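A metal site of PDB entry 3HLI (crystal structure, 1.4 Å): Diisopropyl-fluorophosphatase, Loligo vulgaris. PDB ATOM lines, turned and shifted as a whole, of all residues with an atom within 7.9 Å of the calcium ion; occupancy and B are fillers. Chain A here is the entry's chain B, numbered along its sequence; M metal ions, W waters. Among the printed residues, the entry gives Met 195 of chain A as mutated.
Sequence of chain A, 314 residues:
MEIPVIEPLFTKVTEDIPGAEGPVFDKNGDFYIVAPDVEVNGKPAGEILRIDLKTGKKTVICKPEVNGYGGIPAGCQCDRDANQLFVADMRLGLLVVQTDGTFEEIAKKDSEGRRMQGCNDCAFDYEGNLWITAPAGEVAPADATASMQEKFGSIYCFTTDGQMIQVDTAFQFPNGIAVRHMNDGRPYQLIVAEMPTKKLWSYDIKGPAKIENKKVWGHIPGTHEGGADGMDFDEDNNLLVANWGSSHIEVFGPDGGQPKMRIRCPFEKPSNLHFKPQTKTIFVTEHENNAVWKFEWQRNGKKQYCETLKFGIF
The calcium ion is bound by OD1 of Asn 175, OE2 of Glu 21, OD1 of Asp 229, water W1, OD1 of Asn 120 and water W2.
The calcium ion has six donor atoms within binding distance.
Four residues have an atom within 4 Å of the calcium ion: Glu 21, Asn 120, Asn 175 and Asp 229.
The nearest printed residue that does not touch the calcium ion is Asn 272 (4.4 Å).
Water W1 bridges the side-chain carboxylate (OD2) of Asp 121 (2.7 Å) and the backbone NH (N) of Gly 230 (3.4 Å).
The side-chain amide nitrogen (ND2) of Asn 272 sits at hydrogen-bond distance from the side-chain carboxylate (OE1) of Glu 21, at 2.8 Å.
The backbone carbonyl oxygen (O) of Asn 175 lies within hydrogen-bond range of the side-chain hydroxyl (OG1) of Thr 133 (2.7 Å).
The backbone NH of Asn 120 lies within hydrogen-bond range of the backbone carbonyl oxygen of Thr 133, at 2.9 Å.
N of Gly 75 sits at hydrogen-bond distance from O of Asn 120, at 3.1 Å.
The backbone carbonyl oxygen (O) of Asp 229 sits close to the backbone NH (N) of Gly 176.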
ATOM      1  N   GLY A  19      20.183  16.383   0.792  1.00  0.00           N
ATOM      2  CA  GLY A  19      20.819  16.044  -0.471  1.00  0.00           C
ATOM      3  C   GLY A  19      22.297  15.753  -0.359  1.00  0.00           C
ATOM      4  O   GLY A  19      23.027  15.868  -1.345  1.00  0.00           O
ATOM      5  N   ALA A  20      22.738  15.359   0.844  1.00  0.00           N
ATOM      6  CA  ALA A  20      24.139  15.044   1.140  1.00  0.00           C
ATOM      7  C   ALA A  20      24.907  14.579  -0.089  1.00  0.00           C
ATOM      8  O   ALA A  20      24.564  13.573  -0.712  1.00  0.00           O
ATOM      9  CB  ALA A  20      24.202  13.984   2.229  1.00  0.00           C
ATOM     10  N   GLU A  21      25.967  15.314  -0.422  1.00  0.00           N
ATOM     11  CA  GLU A  21      26.771  15.035  -1.607  1.00  0.00           C
ATOM     12  C   GLU A  21      28.187  15.595  -1.474  1.00  0.00           C
ATOM     13  O   GLU A  21      28.573  16.118  -0.427  1.00  0.00           O
ATOM     14  CB  GLU A  21      26.107  15.667  -2.835  1.00  0.00           C
ATOM     15  CG  GLU A  21      25.437  14.690  -3.789  1.00  0.00           C
ATOM     16  CD  GLU A  21      26.412  14.051  -4.759  1.00  0.00           C
ATOM     17  OE1 GLU A  21      27.628  14.101  -4.498  1.00  0.00           O
ATOM     18  OE2 GLU A  21      25.954  13.481  -5.771  1.00  0.00           O
ATOM     19  N   GLY A  22      28.946  15.452  -2.556  1.00  0.00           N
ATOM     20  CA  GLY A  22      30.299  15.970  -2.638  1.00  0.00           C
ATOM     21  C   GLY A  22      31.260  15.776  -1.478  1.00  0.00           C
ATOM     22  O   GLY A  22      31.914  16.740  -1.062  1.00  0.00           O
ATOM     23  N   PRO A  36      23.113  20.242  -1.397  1.00  0.00           N
ATOM     24  CA  PRO A  36      22.453  20.858  -2.543  1.00  0.00           C
ATOM     25  C   PRO A  36      20.944  21.001  -2.441  1.00  0.00           C
ATOM     26  O   PRO A  36      20.355  21.852  -3.098  1.00  0.00           O
ATOM     27  CB  PRO A  36      22.845  19.936  -3.693  1.00  0.00           C
ATOM     28  CG  PRO A  36      22.969  18.588  -3.028  1.00  0.00           C
ATOM     29  CD  PRO A  36      23.720  18.950  -1.758  1.00  0.00           C
ATOM     30  N   ALA A  74      26.985  20.694  -5.440  1.00  0.00           N
ATOM     31  CA  ALA A  74      26.738  19.259  -5.519  1.00  0.00           C
ATOM     32  C   ALA A  74      27.954  18.329  -5.564  1.00  0.00           C
ATOM     33  O   ALA A  74      27.816  17.153  -5.246  1.00  0.00           O
ATOM     34  CB  ALA A  74      25.837  18.972  -6.722  1.00  0.00           C
ATOM     35  N   GLY A  75      29.113  18.839  -5.970  1.00  0.00           N
ATOM     36  CA  GLY A  75      30.281  17.978  -6.049  1.00  0.00           C
ATOM     37  C   GLY A  75      31.547  18.763  -5.788  1.00  0.00           C
ATOM     38  O   GLY A  75      31.613  19.958  -6.081  1.00  0.00           O
ATOM     39  N   MET A  90      24.944  23.200  -9.317  1.00  0.00           N
ATOM     40  CA  MET A  90      23.851  23.050 -10.274  1.00  0.00           C
ATOM     41  C   MET A  90      23.181  24.350 -10.707  1.00  0.00           C
ATOM     42  O   MET A  90      22.474  24.372 -11.722  1.00  0.00           O
ATOM     43  CB  MET A  90      22.808  22.073  -9.708  1.00  0.00           C
ATOM     44  CG  MET A  90      23.311  20.625  -9.586  1.00  0.00           C
ATOM     45  SD  MET A  90      23.378  19.712 -11.148  1.00  0.00           S
ATOM     46  CE  MET A  90      21.656  19.355 -11.382  1.00  0.00           C
ATOM     47  N   CYS A 119      26.519  22.575 -12.997  1.00  0.00           N
ATOM     48  CA  CYS A 119      27.371  21.390 -12.852  1.00  0.00           C
ATOM     49  C   CYS A 119      27.028  20.524 -11.648  1.00  0.00           C
ATOM     50  O   CYS A 119      26.495  21.007 -10.649  1.00  0.00           O
ATOM     51  CB  CYS A 119      28.832  21.839 -12.805  1.00  0.00           C
ATOM     52  SG  CYS A 119      29.348  22.717 -14.304  1.00  0.00           S
ATOM     53  N   ASN A 120      27.379  19.243 -11.753  1.00  0.00           N
ATOM     54  CA  ASN A 120      27.068  18.271 -10.700  1.00  0.00           C
ATOM     55  C   ASN A 120      28.281  17.686  -9.964  1.00  0.00           C
ATOM     56  O   ASN A 120      28.321  17.671  -8.729  1.00  0.00           O
ATOM     57  CB  ASN A 120      26.228  17.150 -11.300  1.00  0.00           C
ATOM     58  CG  ASN A 120      25.699  16.193 -10.254  1.00  0.00           C
ATOM     59  OD1 ASN A 120      26.454  15.473  -9.632  1.00  0.00           O
ATOM     60  ND2 ASN A 120      24.390  16.194 -10.075  1.00  0.00           N
ATOM     61  N   ASP A 121      29.257  17.184 -10.703  1.00  0.00           N
ATOM     62  CA  ASP A 121      30.445  16.611 -10.061  1.00  0.00           C
ATOM     63  C   ASP A 121      31.660  16.902 -10.923  1.00  0.00           C
ATOM     64  O   ASP A 121      31.551  17.356 -12.065  1.00  0.00           O
ATOM     65  CB  ASP A 121      30.272  15.090  -9.855  1.00  0.00           C
ATOM     66  CG  ASP A 121      31.043  14.566  -8.646  1.00  0.00           C
ATOM     67  OD1 ASP A 121      31.830  15.332  -8.048  1.00  0.00           O
ATOM     68  OD2 ASP A 121      30.862  13.384  -8.283  1.00  0.00           O
ATOM     69  N   CYS A 122      32.841  16.668 -10.367  1.00  0.00           N
ATOM     70  CA  CYS A 122      34.059  16.919 -11.111  1.00  0.00           C
ATOM     71  C   CYS A 122      35.192  16.045 -10.630  1.00  0.00           C
ATOM     72  O   CYS A 122      35.154  15.505  -9.524  1.00  0.00           O
ATOM     73  CB  CYS A 122      34.440  18.407 -11.002  1.00  0.00           C
ATOM     74  SG  CYS A 122      34.613  19.066  -9.315  1.00  0.00           S
ATOM     75  N   THR A 133      30.890  17.389 -14.959  1.00  0.00           N
ATOM     76  CA  THR A 133      29.626  16.997 -15.557  1.00  0.00           C
ATOM     77  C   THR A 133      28.641  18.148 -15.352  1.00  0.00           C
ATOM     78  O   THR A 133      28.632  18.791 -14.296  1.00  0.00           O
ATOM     79  CB  THR A 133      29.031  15.714 -14.932  1.00  0.00           C
ATOM     80  OG1 THR A 133      28.869  15.906 -13.524  1.00  0.00           O
ATOM     81  CG2 THR A 133      29.954  14.534 -15.184  1.00  0.00           C
ATOM     82  N   PRO A 135      24.716  18.366 -15.935  1.00  0.00           N
ATOM     83  CA  PRO A 135      23.393  17.852 -16.286  1.00  0.00           C
ATOM     84  C   PRO A 135      22.264  18.893 -16.266  1.00  0.00           C
ATOM     85  O   PRO A 135      21.207  18.674 -16.854  1.00  0.00           O
ATOM     86  CB  PRO A 135      23.173  16.768 -15.241  1.00  0.00           C
ATOM     87  CG  PRO A 135      23.830  17.365 -14.026  1.00  0.00           C
ATOM     88  CD  PRO A 135      25.123  17.922 -14.598  1.00  0.00           C
ATOM     89  N   PHE A 173      21.582  13.376 -18.303  1.00  0.00           N
ATOM     90  CA  PHE A 173      21.987  13.552 -16.915  1.00  0.00           C
ATOM     91  C   PHE A 173      23.333  12.952 -16.526  1.00  0.00           C
ATOM     92  O   PHE A 173      23.408  11.965 -15.776  1.00  0.00           O
ATOM     93  CB  PHE A 173      20.901  13.055 -15.969  1.00  0.00           C
ATOM     94  CG  PHE A 173      20.774  13.904 -14.736  1.00  0.00           C
ATOM     95  CD1 PHE A 173      21.699  13.819 -13.711  1.00  0.00           C
ATOM     96  CD2 PHE A 173      19.770  14.849 -14.655  1.00  0.00           C
ATOM     97  CE1 PHE A 173      21.634  14.661 -12.614  1.00  0.00           C
ATOM     98  CE2 PHE A 173      19.684  15.704 -13.560  1.00  0.00           C
ATOM     99  CZ  PHE A 173      20.623  15.610 -12.539  1.00  0.00           C
ATOM    100  N   PRO A 174      24.426  13.531 -17.042  1.00  0.00           N
ATOM    101  CA  PRO A 174      25.760  13.035 -16.705  1.00  0.00           C
ATOM    102  C   PRO A 174      25.908  13.358 -15.217  1.00  0.00           C
ATOM    103  O   PRO A 174      25.494  14.439 -14.764  1.00  0.00           O
ATOM    104  CB  PRO A 174      26.671  13.884 -17.593  1.00  0.00           C
ATOM    105  CG  PRO A 174      25.879  15.156 -17.798  1.00  0.00           C
ATOM    106  CD  PRO A 174      24.480  14.649 -17.996  1.00  0.00           C
ATOM    107  N   ASN A 175      26.472  12.443 -14.442  1.00  0.00           N
ATOM    108  CA  ASN A 175      26.565  12.674 -13.016  1.00  0.00           C
ATOM    109  C   ASN A 175      27.987  12.451 -12.492  1.00  0.00           C
ATOM    110  O   ASN A 175      28.791  13.372 -12.508  1.00  0.00           O
ATOM    111  CB  ASN A 175      25.560  11.777 -12.296  1.00  0.00           C
ATOM    112  CG  ASN A 175      25.170  12.317 -10.936  1.00  0.00           C
ATOM    113  OD1 ASN A 175      26.026  12.750 -10.187  1.00  0.00           O
ATOM    114  ND2 ASN A 175      23.879  12.311 -10.635  1.00  0.00           N
ATOM    115  N   GLY A 176      28.290  11.239 -12.035  1.00  0.00           N
ATOM    116  CA  GLY A 176      29.629  10.958 -11.570  1.00  0.00           C
ATOM    117  C   GLY A 176      30.646  11.005 -12.705  1.00  0.00           C
ATOM    118  O   GLY A 176      30.297  10.835 -13.877  1.00  0.00           O
ATOM    119  N   ILE A 177      31.903  11.230 -12.365  1.00  0.00           N
ATOM    120  CA  ILE A 177      32.966  11.296 -13.360  1.00  0.00           C
ATOM    121  C   ILE A 177      34.289  10.914 -12.699  1.00  0.00           C
ATOM    122  O   ILE A 177      34.476  11.131 -11.511  1.00  0.00           O
ATOM    123  CB  ILE A 177      33.011  12.733 -13.977  1.00  0.00           C
ATOM    124  CG1 ILE A 177      34.015  12.796 -15.119  1.00  0.00           C
ATOM    125  CG2 ILE A 177      33.323  13.753 -12.893  1.00  0.00           C
ATOM    126  CD1 ILE A 177      33.826  14.020 -16.000  1.00  0.00           C
ATOM    127  N   MET A 195      23.448   8.731 -15.521  1.00  0.00           N
ATOM    128  CA  MET A 195      22.571   8.119 -14.539  1.00  0.00           C
ATOM    129  C   MET A 195      21.359   7.289 -14.952  1.00  0.00           C
ATOM    130  O   MET A 195      21.339   6.080 -14.767  1.00  0.00           O
ATOM    131  CB  MET A 195      22.142   9.160 -13.499  1.00  0.00           C
ATOM    132  CG  MET A 195      21.317   8.545 -12.383  1.00  0.00           C
ATOM    133  SD  MET A 195      20.950   9.704 -11.063  1.00  0.00           S
ATOM    134  CE  MET A 195      22.174   9.240  -9.829  1.00  0.00           C
ATOM    135  N   ALA A 228      23.931   5.273 -11.722  1.00  0.00           N
ATOM    136  CA  ALA A 228      25.236   5.728 -11.258  1.00  0.00           C
ATOM    137  C   ALA A 228      25.253   7.193 -10.877  1.00  0.00           C
ATOM    138  O   ALA A 228      24.858   8.056 -11.644  1.00  0.00           O
ATOM    139  CB  ALA A 228      26.297   5.455 -12.318  1.00  0.00           C
ATOM    140  N   ASP A 229      25.714   7.462  -9.654  1.00  0.00           N
ATOM    141  CA  ASP A 229      25.840   8.824  -9.165  1.00  0.00           C
ATOM    142  C   ASP A 229      27.353   9.088  -9.067  1.00  0.00           C
ATOM    143  O   ASP A 229      28.020   9.115 -10.103  1.00  0.00           O
ATOM    144  CB  ASP A 229      25.148   8.976  -7.797  1.00  0.00           C
ATOM    145  CG  ASP A 229      24.764  10.414  -7.493  1.00  0.00           C
ATOM    146  OD1 ASP A 229      25.504  11.320  -7.915  1.00  0.00           O
ATOM    147  OD2 ASP A 229      23.737  10.640  -6.805  1.00  0.00           O
ATOM    148  N   GLY A 230      27.899   9.240  -7.864  1.00  0.00           N
ATOM    149  CA  GLY A 230      29.319   9.495  -7.716  1.00  0.00           C
ATOM    150  C   GLY A 230      30.216   8.275  -7.851  1.00  0.00           C
ATOM    151  O   GLY A 230      29.759   7.152  -7.697  1.00  0.00           O
ATOM    152  N   MET A 231      31.495   8.511  -8.124  1.00  0.00           N
ATOM    153  CA  MET A 231      32.458   7.424  -8.298  1.00  0.00           C
ATOM    154  C   MET A 231      33.880   7.831  -7.944  1.00  0.00           C
ATOM    155  O   MET A 231      34.210   9.010  -7.908  1.00  0.00           O
ATOM    156  CB  MET A 231      32.448   6.938  -9.750  1.00  0.00           C
ATOM    157  CG  MET A 231      32.842   8.035 -10.720  1.00  0.00           C
ATOM    158  SD  MET A 231      32.891   7.522 -12.446  1.00  0.00           S
ATOM    159  CE  MET A 231      31.248   6.857 -12.605  1.00  0.00           C
ATOM    160  N   TRP A 244      22.648   4.789  -7.059  1.00  0.00           N
ATOM    161  CA  TRP A 244      21.499   5.407  -6.395  1.00  0.00           C
ATOM    162  C   TRP A 244      20.199   4.650  -6.682  1.00  0.00           C
ATOM    163  O   TRP A 244      19.814   4.493  -7.839  1.00  0.00           O
ATOM    164  CB  TRP A 244      21.384   6.853  -6.879  1.00  0.00           C
ATOM    165  CG  TRP A 244      20.523   7.790  -6.058  1.00  0.00           C
ATOM    166  CD1 TRP A 244      20.950   8.785  -5.229  1.00  0.00           C
ATOM    167  CD2 TRP A 244      19.089   7.885  -6.084  1.00  0.00           C
ATOM    168  NE1 TRP A 244      19.886   9.505  -4.740  1.00  0.00           N
ATOM    169  CE2 TRP A 244      18.724   8.972  -5.247  1.00  0.00           C
ATOM    170  CE3 TRP A 244      18.071   7.172  -6.734  1.00  0.00           C
ATOM    171  CZ2 TRP A 244      17.398   9.363  -5.047  1.00  0.00           C
ATOM    172  CZ3 TRP A 244      16.744   7.547  -6.527  1.00  0.00           C
ATOM    173  CH2 TRP A 244      16.429   8.637  -5.694  1.00  0.00           C
ATOM    174  N   SER A 271      24.736   8.379  -2.792  1.00  0.00           N
ATOM    175  CA  SER A 271      24.904   9.419  -3.808  1.00  0.00           C
ATOM    176  C   SER A 271      26.351   9.626  -4.218  1.00  0.00           C
ATOM    177  O   SER A 271      26.643   9.865  -5.387  1.00  0.00           O
ATOM    178  CB  SER A 271      24.321  10.751  -3.302  1.00  0.00           C
ATOM    179  OG  SER A 271      24.970  11.179  -2.120  1.00  0.00           O
ATOM    180  N   ASN A 272      27.271   9.517  -3.266  1.00  0.00           N
ATOM    181  CA  ASN A 272      28.672   9.712  -3.602  1.00  0.00           C
ATOM    182  C   ASN A 272      29.575   9.097  -2.546  1.00  0.00           C
ATOM    183  O   ASN A 272      29.095   8.595  -1.527  1.00  0.00           O
ATOM    184  CB  ASN A 272      28.984  11.217  -3.745  1.00  0.00           C
ATOM    185  CG  ASN A 272      29.968  11.499  -4.857  1.00  0.00           C
ATOM    186  OD1 ASN A 272      30.867  10.694  -5.122  1.00  0.00           O
ATOM    187  ND2 ASN A 272      29.820  12.647  -5.508  1.00  0.00           N
ATOM    188  N   THR A 285      27.933   9.424   1.134  1.00  0.00           N
ATOM    189  CA  THR A 285      26.804  10.322   1.323  1.00  0.00           C
ATOM    190  C   THR A 285      25.607   9.586   0.726  1.00  0.00           C
ATOM    191  O   THR A 285      25.760   8.819  -0.226  1.00  0.00           O
ATOM    192  CB  THR A 285      27.008  11.671   0.606  1.00  0.00           C
ATOM    193  OG1 THR A 285      27.415  11.441  -0.757  1.00  0.00           O
ATOM    194  CG2 THR A 285      28.075  12.496   1.303  1.00  0.00           C
ATOM    195  N   HIS A 287      21.019   9.752   0.065  1.00  0.00           N
ATOM    196  CA  HIS A 287      19.775  10.500   0.060  1.00  0.00           C
ATOM    197  C   HIS A 287      18.549   9.872   0.707  1.00  0.00           C
ATOM    198  O   HIS A 287      17.480  10.491   0.720  1.00  0.00           O
ATOM    199  CB  HIS A 287      19.456  10.922  -1.371  1.00  0.00           C
ATOM    200  CG  HIS A 287      20.500  11.799  -1.984  1.00  0.00           C
ATOM    201  ND1 HIS A 287      20.572  12.048  -3.341  1.00  0.00           N
ATOM    202  CD2 HIS A 287      21.500  12.528  -1.417  1.00  0.00           C
ATOM    203  CE1 HIS A 287      21.574  12.878  -3.583  1.00  0.00           C
ATOM    204  NE2 HIS A 287      22.152  13.183  -2.432  1.00  0.00           N
HETATM  205 CA    CA M   1      26.305  13.564  -8.053  1.00  0.00          CA
HETATM  206  O   HOH W   1      28.327  12.460  -8.721  1.00  0.00           O
HETATM  207  O   HOH W   2      27.917  15.285  -7.264  1.00  0.00           O
